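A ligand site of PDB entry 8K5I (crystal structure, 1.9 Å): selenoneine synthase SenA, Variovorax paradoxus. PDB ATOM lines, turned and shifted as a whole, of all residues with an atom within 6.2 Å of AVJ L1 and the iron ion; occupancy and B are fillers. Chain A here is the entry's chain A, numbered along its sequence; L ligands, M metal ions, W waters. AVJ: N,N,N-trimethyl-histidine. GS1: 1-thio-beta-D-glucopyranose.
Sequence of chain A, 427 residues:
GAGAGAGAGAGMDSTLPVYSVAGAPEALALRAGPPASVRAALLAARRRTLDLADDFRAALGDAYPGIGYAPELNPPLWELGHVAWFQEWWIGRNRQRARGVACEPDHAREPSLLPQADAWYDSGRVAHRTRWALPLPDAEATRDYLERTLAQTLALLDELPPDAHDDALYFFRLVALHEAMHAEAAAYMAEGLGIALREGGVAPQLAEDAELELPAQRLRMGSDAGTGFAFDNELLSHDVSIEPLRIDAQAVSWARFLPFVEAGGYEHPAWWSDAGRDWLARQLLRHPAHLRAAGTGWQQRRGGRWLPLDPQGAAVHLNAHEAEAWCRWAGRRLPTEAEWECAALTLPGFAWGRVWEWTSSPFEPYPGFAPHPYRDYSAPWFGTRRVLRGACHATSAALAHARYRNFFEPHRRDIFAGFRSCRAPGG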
ATOM      1  N   TRP A  78     -13.077  27.123 -38.940  1.00  0.00           N
ATOM      2  CA  TRP A  78     -13.777  26.387 -37.852  1.00  0.00           C
ATOM      3  C   TRP A  78     -13.276  26.967 -36.528  1.00  0.00           C
ATOM      4  O   TRP A  78     -14.083  27.349 -35.736  1.00  0.00           O
ATOM      5  CB  TRP A  78     -13.564  24.881 -37.932  1.00  0.00           C
ATOM      6  CG  TRP A  78     -14.368  24.225 -36.862  1.00  0.00           C
ATOM      7  CD1 TRP A  78     -15.669  23.838 -36.976  1.00  0.00           C
ATOM      8  CD2 TRP A  78     -13.977  23.984 -35.504  1.00  0.00           C
ATOM      9  NE1 TRP A  78     -16.093  23.321 -35.790  1.00  0.00           N
ATOM     10  CE2 TRP A  78     -15.082  23.370 -34.883  1.00  0.00           C
ATOM     11  CE3 TRP A  78     -12.783  24.158 -34.789  1.00  0.00           C
ATOM     12  CZ2 TRP A  78     -15.051  22.994 -33.547  1.00  0.00           C
ATOM     13  CZ3 TRP A  78     -12.762  23.809 -33.444  1.00  0.00           C
ATOM     14  CH2 TRP A  78     -13.864  23.195 -32.843  1.00  0.00           C
ATOM     15  N   HIS A  82     -15.486  28.710 -33.680  1.00  0.00           N
ATOM     16  CA  HIS A  82     -15.465  28.056 -32.365  1.00  0.00           C
ATOM     17  C   HIS A  82     -15.157  29.104 -31.299  1.00  0.00           C
ATOM     18  O   HIS A  82     -15.703  29.011 -30.196  1.00  0.00           O
ATOM     19  CB  HIS A  82     -14.452  26.909 -32.327  1.00  0.00           C
ATOM     20  CG  HIS A  82     -14.248  26.401 -30.940  1.00  0.00           C
ATOM     21  ND1 HIS A  82     -15.197  25.621 -30.281  1.00  0.00           N
ATOM     22  CD2 HIS A  82     -13.247  26.572 -30.055  1.00  0.00           C
ATOM     23  CE1 HIS A  82     -14.765  25.326 -29.068  1.00  0.00           C
ATOM     24  NE2 HIS A  82     -13.590  25.900 -28.895  1.00  0.00           N
ATOM     25  N   PHE A  86     -17.918  29.760 -28.393  1.00  0.00           N
ATOM     26  CA  PHE A  86     -17.530  29.528 -26.994  1.00  0.00           C
ATOM     27  C   PHE A  86     -17.827  30.784 -26.167  1.00  0.00           C
ATOM     28  O   PHE A  86     -18.408  30.688 -25.070  1.00  0.00           O
ATOM     29  CB  PHE A  86     -16.059  29.086 -26.889  1.00  0.00           C
ATOM     30  CG  PHE A  86     -15.694  28.640 -25.504  1.00  0.00           C
ATOM     31  CD1 PHE A  86     -15.286  29.564 -24.542  1.00  0.00           C
ATOM     32  CD2 PHE A  86     -15.795  27.295 -25.132  1.00  0.00           C
ATOM     33  CE1 PHE A  86     -14.932  29.168 -23.261  1.00  0.00           C
ATOM     34  CE2 PHE A  86     -15.424  26.890 -23.848  1.00  0.00           C
ATOM     35  CZ  PHE A  86     -15.004  27.823 -22.925  1.00  0.00           C
ATOM     36  N   SER A 123     -17.266  21.974 -29.667  1.00  0.00           N
ATOM     37  CA  SER A 123     -16.178  20.976 -29.717  1.00  0.00           C
ATOM     38  C   SER A 123     -16.588  19.694 -28.963  1.00  0.00           C
ATOM     39  O   SER A 123     -15.961  18.690 -29.236  1.00  0.00           O
ATOM     40  CB  SER A 123     -14.883  21.558 -29.219  1.00  0.00           C
ATOM     41  OG  SER A 123     -15.020  22.047 -27.894  1.00  0.00           O
ATOM     42  N   HIS A 178      -9.762  31.126 -22.893  1.00  0.00           N
ATOM     43  CA  HIS A 178     -10.062  30.092 -23.896  1.00  0.00           C
ATOM     44  C   HIS A 178      -9.563  30.585 -25.252  1.00  0.00           C
ATOM     45  O   HIS A 178      -8.929  29.837 -26.013  1.00  0.00           O
ATOM     46  CB  HIS A 178     -11.569  29.775 -23.935  1.00  0.00           C
ATOM     47  CG  HIS A 178     -11.934  28.877 -25.062  1.00  0.00           C
ATOM     48  ND1 HIS A 178     -12.539  29.339 -26.215  1.00  0.00           N
ATOM     49  CD2 HIS A 178     -11.705  27.564 -25.221  1.00  0.00           C
ATOM     50  CE1 HIS A 178     -12.719  28.313 -27.024  1.00  0.00           C
ATOM     51  NE2 HIS A 178     -12.222  27.199 -26.437  1.00  0.00           N
ATOM     52  N   MET A 181      -5.868  30.437 -25.582  1.00  0.00           N
ATOM     53  CA  MET A 181      -5.434  29.059 -25.857  1.00  0.00           C
ATOM     54  C   MET A 181      -5.618  28.734 -27.340  1.00  0.00           C
ATOM     55  O   MET A 181      -4.698  28.145 -27.909  1.00  0.00           O
ATOM     56  CB  MET A 181      -6.169  28.052 -24.967  1.00  0.00           C
ATOM     57  CG  MET A 181      -5.684  28.108 -23.543  1.00  0.00           C
ATOM     58  SD  MET A 181      -6.500  26.865 -22.464  1.00  0.00           S
ATOM     59  CE  MET A 181      -8.193  27.409 -22.497  1.00  0.00           C
ATOM     60  N   HIS A 182      -6.704  29.156 -27.988  1.00  0.00           N
ATOM     61  CA  HIS A 182      -6.931  28.894 -29.417  1.00  0.00           C
ATOM     62  C   HIS A 182      -5.918  29.714 -30.248  1.00  0.00           C
ATOM     63  O   HIS A 182      -5.569  29.249 -31.322  1.00  0.00           O
ATOM     64  CB  HIS A 182      -8.411  29.150 -29.788  1.00  0.00           C
ATOM     65  CG  HIS A 182      -9.256  27.960 -29.495  1.00  0.00           C
ATOM     66  ND1 HIS A 182      -9.373  26.919 -30.375  1.00  0.00           N
ATOM     67  CD2 HIS A 182      -9.951  27.617 -28.387  1.00  0.00           C
ATOM     68  CE1 HIS A 182     -10.102  25.962 -29.819  1.00  0.00           C
ATOM     69  NE2 HIS A 182     -10.499  26.383 -28.611  1.00  0.00           N
ATOM     70  N   ALA A 185      -2.867  27.734 -30.410  1.00  0.00           N
ATOM     71  CA  ALA A 185      -3.141  26.546 -31.256  1.00  0.00           C
ATOM     72  C   ALA A 185      -3.005  26.949 -32.736  1.00  0.00           C
ATOM     73  O   ALA A 185      -2.388  26.179 -33.530  1.00  0.00           O
ATOM     74  CB  ALA A 185      -4.491  25.977 -30.942  1.00  0.00           C
ATOM     75  N   TYR A 188       0.807  26.981 -33.361  1.00  0.00           N
ATOM     76  CA  TYR A 188       1.491  25.666 -33.552  1.00  0.00           C
ATOM     77  C   TYR A 188       0.915  24.923 -34.767  1.00  0.00           C
ATOM     78  O   TYR A 188       1.675  24.238 -35.454  1.00  0.00           O
ATOM     79  CB  TYR A 188       1.567  24.796 -32.308  1.00  0.00           C
ATOM     80  CG  TYR A 188       0.311  24.219 -31.703  1.00  0.00           C
ATOM     81  CD1 TYR A 188      -0.365  23.164 -32.274  1.00  0.00           C
ATOM     82  CD2 TYR A 188      -0.074  24.617 -30.431  1.00  0.00           C
ATOM     83  CE1 TYR A 188      -1.482  22.604 -31.676  1.00  0.00           C
ATOM     84  CE2 TYR A 188      -1.178  24.070 -29.810  1.00  0.00           C
ATOM     85  CZ  TYR A 188      -1.870  23.039 -30.415  1.00  0.00           C
ATOM     86  OH  TYR A 188      -2.978  22.519 -29.815  1.00  0.00           O
ATOM     87  N   TYR A 374     -17.558  24.473 -17.574  1.00  0.00           N
ATOM     88  CA  TYR A 374     -17.021  23.833 -18.819  1.00  0.00           C
ATOM     89  C   TYR A 374     -16.427  22.479 -18.426  1.00  0.00           C
ATOM     90  O   TYR A 374     -15.192  22.312 -18.221  1.00  0.00           O
ATOM     91  CB  TYR A 374     -16.052  24.778 -19.535  1.00  0.00           C
ATOM     92  CG  TYR A 374     -15.394  24.196 -20.759  1.00  0.00           C
ATOM     93  CD1 TYR A 374     -16.002  23.189 -21.501  1.00  0.00           C
ATOM     94  CD2 TYR A 374     -14.168  24.671 -21.186  1.00  0.00           C
ATOM     95  CE1 TYR A 374     -15.389  22.644 -22.621  1.00  0.00           C
ATOM     96  CE2 TYR A 374     -13.561  24.153 -22.317  1.00  0.00           C
ATOM     97  CZ  TYR A 374     -14.169  23.133 -23.039  1.00  0.00           C
ATOM     98  OH  TYR A 374     -13.573  22.606 -24.131  1.00  0.00           O
ATOM     99  N   TYR A 377     -13.286  20.500 -19.883  1.00  0.00           N
ATOM    100  CA  TYR A 377     -11.964  21.173 -20.040  1.00  0.00           C
ATOM    101  C   TYR A 377     -10.839  20.221 -19.567  1.00  0.00           C
ATOM    102  O   TYR A 377      -9.796  20.059 -20.288  1.00  0.00           O
ATOM    103  CB  TYR A 377     -11.875  22.528 -19.328  1.00  0.00           C
ATOM    104  CG  TYR A 377     -10.513  23.163 -19.437  1.00  0.00           C
ATOM    105  CD1 TYR A 377     -10.021  23.603 -20.662  1.00  0.00           C
ATOM    106  CD2 TYR A 377      -9.691  23.294 -18.320  1.00  0.00           C
ATOM    107  CE1 TYR A 377      -8.766  24.170 -20.770  1.00  0.00           C
ATOM    108  CE2 TYR A 377      -8.432  23.857 -18.396  1.00  0.00           C
ATOM    109  CZ  TYR A 377      -7.948  24.279 -19.633  1.00  0.00           C
ATOM    110  OH  TYR A 377      -6.681  24.792 -19.718  1.00  0.00           O
ATOM    111  N   TRP A 381      -9.559  14.072 -19.751  1.00  0.00           N
ATOM    112  CA  TRP A 381      -8.159  13.938 -20.248  1.00  0.00           C
ATOM    113  C   TRP A 381      -7.227  13.398 -19.160  1.00  0.00           C
ATOM    114  O   TRP A 381      -6.030  13.261 -19.438  1.00  0.00           O
ATOM    115  CB  TRP A 381      -7.678  15.301 -20.818  1.00  0.00           C
ATOM    116  CG  TRP A 381      -8.765  15.997 -21.588  1.00  0.00           C
ATOM    117  CD1 TRP A 381      -9.373  17.180 -21.261  1.00  0.00           C
ATOM    118  CD2 TRP A 381      -9.450  15.513 -22.752  1.00  0.00           C
ATOM    119  NE1 TRP A 381     -10.389  17.448 -22.129  1.00  0.00           N
ATOM    120  CE2 TRP A 381     -10.453  16.464 -23.071  1.00  0.00           C
ATOM    121  CE3 TRP A 381      -9.314  14.388 -23.567  1.00  0.00           C
ATOM    122  CZ2 TRP A 381     -11.273  16.320 -24.178  1.00  0.00           C
ATOM    123  CZ3 TRP A 381     -10.172  14.226 -24.640  1.00  0.00           C
ATOM    124  CH2 TRP A 381     -11.130  15.199 -24.952  1.00  0.00           C
ATOM    125  N   TYR A 404      -0.374  27.074 -13.904  1.00  0.00           N
ATOM    126  CA  TYR A 404      -1.149  26.556 -15.053  1.00  0.00           C
ATOM    127  C   TYR A 404      -0.692  25.146 -15.365  1.00  0.00           C
ATOM    128  O   TYR A 404       0.553  24.908 -15.441  1.00  0.00           O
ATOM    129  CB  TYR A 404      -0.956  27.462 -16.271  1.00  0.00           C
ATOM    130  CG  TYR A 404      -1.792  27.000 -17.430  1.00  0.00           C
ATOM    131  CD1 TYR A 404      -3.120  27.380 -17.551  1.00  0.00           C
ATOM    132  CD2 TYR A 404      -1.229  26.219 -18.406  1.00  0.00           C
ATOM    133  CE1 TYR A 404      -3.889  26.907 -18.598  1.00  0.00           C
ATOM    134  CE2 TYR A 404      -1.975  25.759 -19.478  1.00  0.00           C
ATOM    135  CZ  TYR A 404      -3.303  26.125 -19.579  1.00  0.00           C
ATOM    136  OH  TYR A 404      -4.001  25.695 -20.634  1.00  0.00           O
ATOM    137  N   ARG A 405      -1.623  24.211 -15.494  1.00  0.00           N
ATOM    138  CA  ARG A 405      -1.268  22.853 -15.915  1.00  0.00           C
ATOM    139  C   ARG A 405      -1.648  22.678 -17.392  1.00  0.00           C
ATOM    140  O   ARG A 405      -2.860  22.727 -17.695  1.00  0.00           O
ATOM    141  CB  ARG A 405      -1.986  21.859 -15.012  1.00  0.00           C
ATOM    142  CG  ARG A 405      -1.768  22.143 -13.524  1.00  0.00           C
ATOM    143  CD  ARG A 405      -2.617  21.162 -12.755  1.00  0.00           C
ATOM    144  NE  ARG A 405      -2.042  19.827 -12.712  1.00  0.00           N
ATOM    145  CZ  ARG A 405      -2.765  18.754 -12.419  1.00  0.00           C
ATOM    146  NH1 ARG A 405      -4.061  18.868 -12.178  1.00  0.00           N
ATOM    147  NH2 ARG A 405      -2.189  17.576 -12.355  1.00  0.00           N
ATOM    148  N   ASN A 406      -0.680  22.456 -18.268  1.00  0.00           N
ATOM    149  CA  ASN A 406      -0.994  22.090 -19.662  1.00  0.00           C
ATOM    150  C   ASN A 406      -1.020  20.560 -19.702  1.00  0.00           C
ATOM    151  O   ASN A 406      -0.411  19.929 -18.833  1.00  0.00           O
ATOM    152  CB  ASN A 406      -0.068  22.764 -20.649  1.00  0.00           C
ATOM    153  CG  ASN A 406      -0.720  22.951 -22.002  1.00  0.00           C
ATOM    154  OD1 ASN A 406      -1.845  22.492 -22.227  1.00  0.00           O
ATOM    155  ND2 ASN A 406      -0.045  23.638 -22.901  1.00  0.00           N
ATOM    156  N   PHE A 407      -1.695  19.986 -20.681  1.00  0.00           N
ATOM    157  CA  PHE A 407      -1.975  18.536 -20.736  1.00  0.00           C
ATOM    158  C   PHE A 407      -2.167  18.135 -22.210  1.00  0.00           C
ATOM    159  O   PHE A 407      -3.116  18.566 -22.884  1.00  0.00           O
ATOM    160  CB  PHE A 407      -3.140  18.165 -19.801  1.00  0.00           C
ATOM    161  CG  PHE A 407      -4.370  19.038 -19.927  1.00  0.00           C
ATOM    162  CD1 PHE A 407      -4.462  20.243 -19.246  1.00  0.00           C
ATOM    163  CD2 PHE A 407      -5.460  18.620 -20.684  1.00  0.00           C
ATOM    164  CE1 PHE A 407      -5.620  21.006 -19.339  1.00  0.00           C
ATOM    165  CE2 PHE A 407      -6.619  19.383 -20.767  1.00  0.00           C
ATOM    166  CZ  PHE A 407      -6.697  20.569 -20.094  1.00  0.00           C
ATOM    167  N   PHE A 408      -1.255  17.292 -22.677  1.00  0.00           N
ATOM    168  CA  PHE A 408      -1.252  16.660 -24.015  1.00  0.00           C
ATOM    169  C   PHE A 408      -0.788  15.217 -23.879  1.00  0.00           C
ATOM    170  O   PHE A 408      -0.046  14.908 -22.957  1.00  0.00           O
ATOM    171  CB  PHE A 408      -0.351  17.447 -24.966  1.00  0.00           C
ATOM    172  CG  PHE A 408      -0.967  18.713 -25.514  1.00  0.00           C
ATOM    173  CD1 PHE A 408      -1.915  18.640 -26.522  1.00  0.00           C
ATOM    174  CD2 PHE A 408      -0.605  19.953 -25.008  1.00  0.00           C
ATOM    175  CE1 PHE A 408      -2.490  19.801 -27.042  1.00  0.00           C
ATOM    176  CE2 PHE A 408      -1.169  21.109 -25.536  1.00  0.00           C
ATOM    177  CZ  PHE A 408      -2.092  21.035 -26.560  1.00  0.00           C
HETATM  178  CAA AVJ L   1      -5.264  23.240 -22.379  1.00  0.00           C
HETATM  179  CAB AVJ L   1      -4.827  21.157 -23.566  1.00  0.00           C
HETATM  180  CAC AVJ L   1      -4.235  23.320 -24.565  1.00  0.00           C
HETATM  181  OAH AVJ L   1      -7.467  20.799 -25.761  1.00  0.00           O
HETATM  182  OAL AVJ L   1      -5.813  22.004 -26.603  1.00  0.00           O
HETATM  183  CAM AVJ L   1      -9.187  24.807 -26.093  1.00  0.00           C
HETATM  184  CAP AVJ L   1      -7.139  23.989 -24.739  1.00  0.00           C
HETATM  185  NAR AVJ L   1      -9.549  23.325 -24.538  1.00  0.00           N
HETATM  186  NAT AVJ L   1     -10.525  24.551 -26.052  1.00  0.00           N
HETATM  187  CAX AVJ L   1      -6.637  21.715 -25.710  1.00  0.00           C
HETATM  188  CAY AVJ L   1      -8.565  24.082 -25.140  1.00  0.00           C
HETATM  189  CAZ AVJ L   1     -10.696  23.660 -25.115  1.00  0.00           C
HETATM  190  CBC AVJ L   1      -6.638  22.566 -24.424  1.00  0.00           C
HETATM  191  NBE AVJ L   1      -5.253  22.595 -23.736  1.00  0.00           N
HETATM  192  C1  GS1 L   2     -10.181  22.583 -28.585  1.00  0.00           C
HETATM  193  S1  GS1 L   2     -11.822  23.420 -28.650  1.00  0.00           S
HETATM  194  C2  GS1 L   2     -10.264  21.106 -28.991  1.00  0.00           C
HETATM  195  O2  GS1 L   2     -11.340  20.392 -28.323  1.00  0.00           O
HETATM  196  C3  GS1 L   2      -8.888  20.451 -28.749  1.00  0.00           C
HETATM  197  O3  GS1 L   2      -8.992  19.032 -29.047  1.00  0.00           O
HETATM  198  C4  GS1 L   2      -7.710  21.148 -29.459  1.00  0.00           C
HETATM  199  O4  GS1 L   2      -6.416  20.665 -28.866  1.00  0.00           O
HETATM  200  C5  GS1 L   2      -7.854  22.696 -29.377  1.00  0.00           C
HETATM  201  O5  GS1 L   2      -9.214  23.140 -29.514  1.00  0.00           O
HETATM  202  C6  GS1 L   2      -6.990  23.454 -30.406  1.00  0.00           C
HETATM  203  O6  GS1 L   2      -7.527  23.417 -31.738  1.00  0.00           O
HETATM  204 FE    FE M   1     -11.981  25.427 -27.506  1.00  0.00          FE
HETATM  205  O   HOH W   1      -4.665  23.737 -28.032  1.00  0.00           O
HETATM  206  O   HOH W   2      -3.464  25.811 -26.732  1.00  0.00           O
HETATM  207  O   HOH W   3      -1.393  25.228 -25.100  1.00  0.00           O
HETATM  208  O   HOH W   4      -9.413  21.069 -22.782  1.00  0.00           O
HETATM  209  O   HOH W   5     -13.524  24.494 -26.189  1.00  0.00           O
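S1 of GS1 L2 lies close to OG of Ser 123 (3.6 Å).
The side-chain hydroxyl of Tyr 404 is in hydrogen-bond range of the side-chain sulfur of Met 181, 3.3 Å away.
The indole nitrogen (NE1) of Trp 381 sits close to the backbone carbonyl oxygen (O) of Tyr 377, 3.2 Å away.
OH of Tyr 377 sits at hydrogen-bond distance from SD of Met 181 (3.4 Å).
OH of Tyr 377 lies within hydrogen-bond range of OH of Tyr 404 (3.0 Å).
Merely in contact with AVJ L1: Met 181, Tyr 374, Tyr 377, Tyr 404, Asn 406, Phe 407 and Phe 408.
Hydrophobic or aromatic side chains that line AVJ L1: His 178, Met 181, His 182, Tyr 377, Phe 407 and Phe 408.
Along chain A the residues within 4 Å of AVJ L1 span positions 178 to 408.
The nearest printed residue that does not touch the iron ion is Ser 123 (4.6 Å).
The iron ion is bound by NE2 of His 182, NE2 of His 178, NE2 of His 82, water W5, NAT of AVJ L1 and S1 of GS1 L2.
The iron ion has six donor atoms within binding distance.
Water W5 bridges the side-chain hydroxyl of Tyr 374 (2.8 Å) and the side-chain hydroxyl of Ser 123 (3.3 Å).
Water W1 bridges OAL of AVJ L1 (2.5 Å) and OH of Tyr 188 (2.7 Å).
Water W4 bridges O of Tyr 377 and NAR of AVJ L1.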
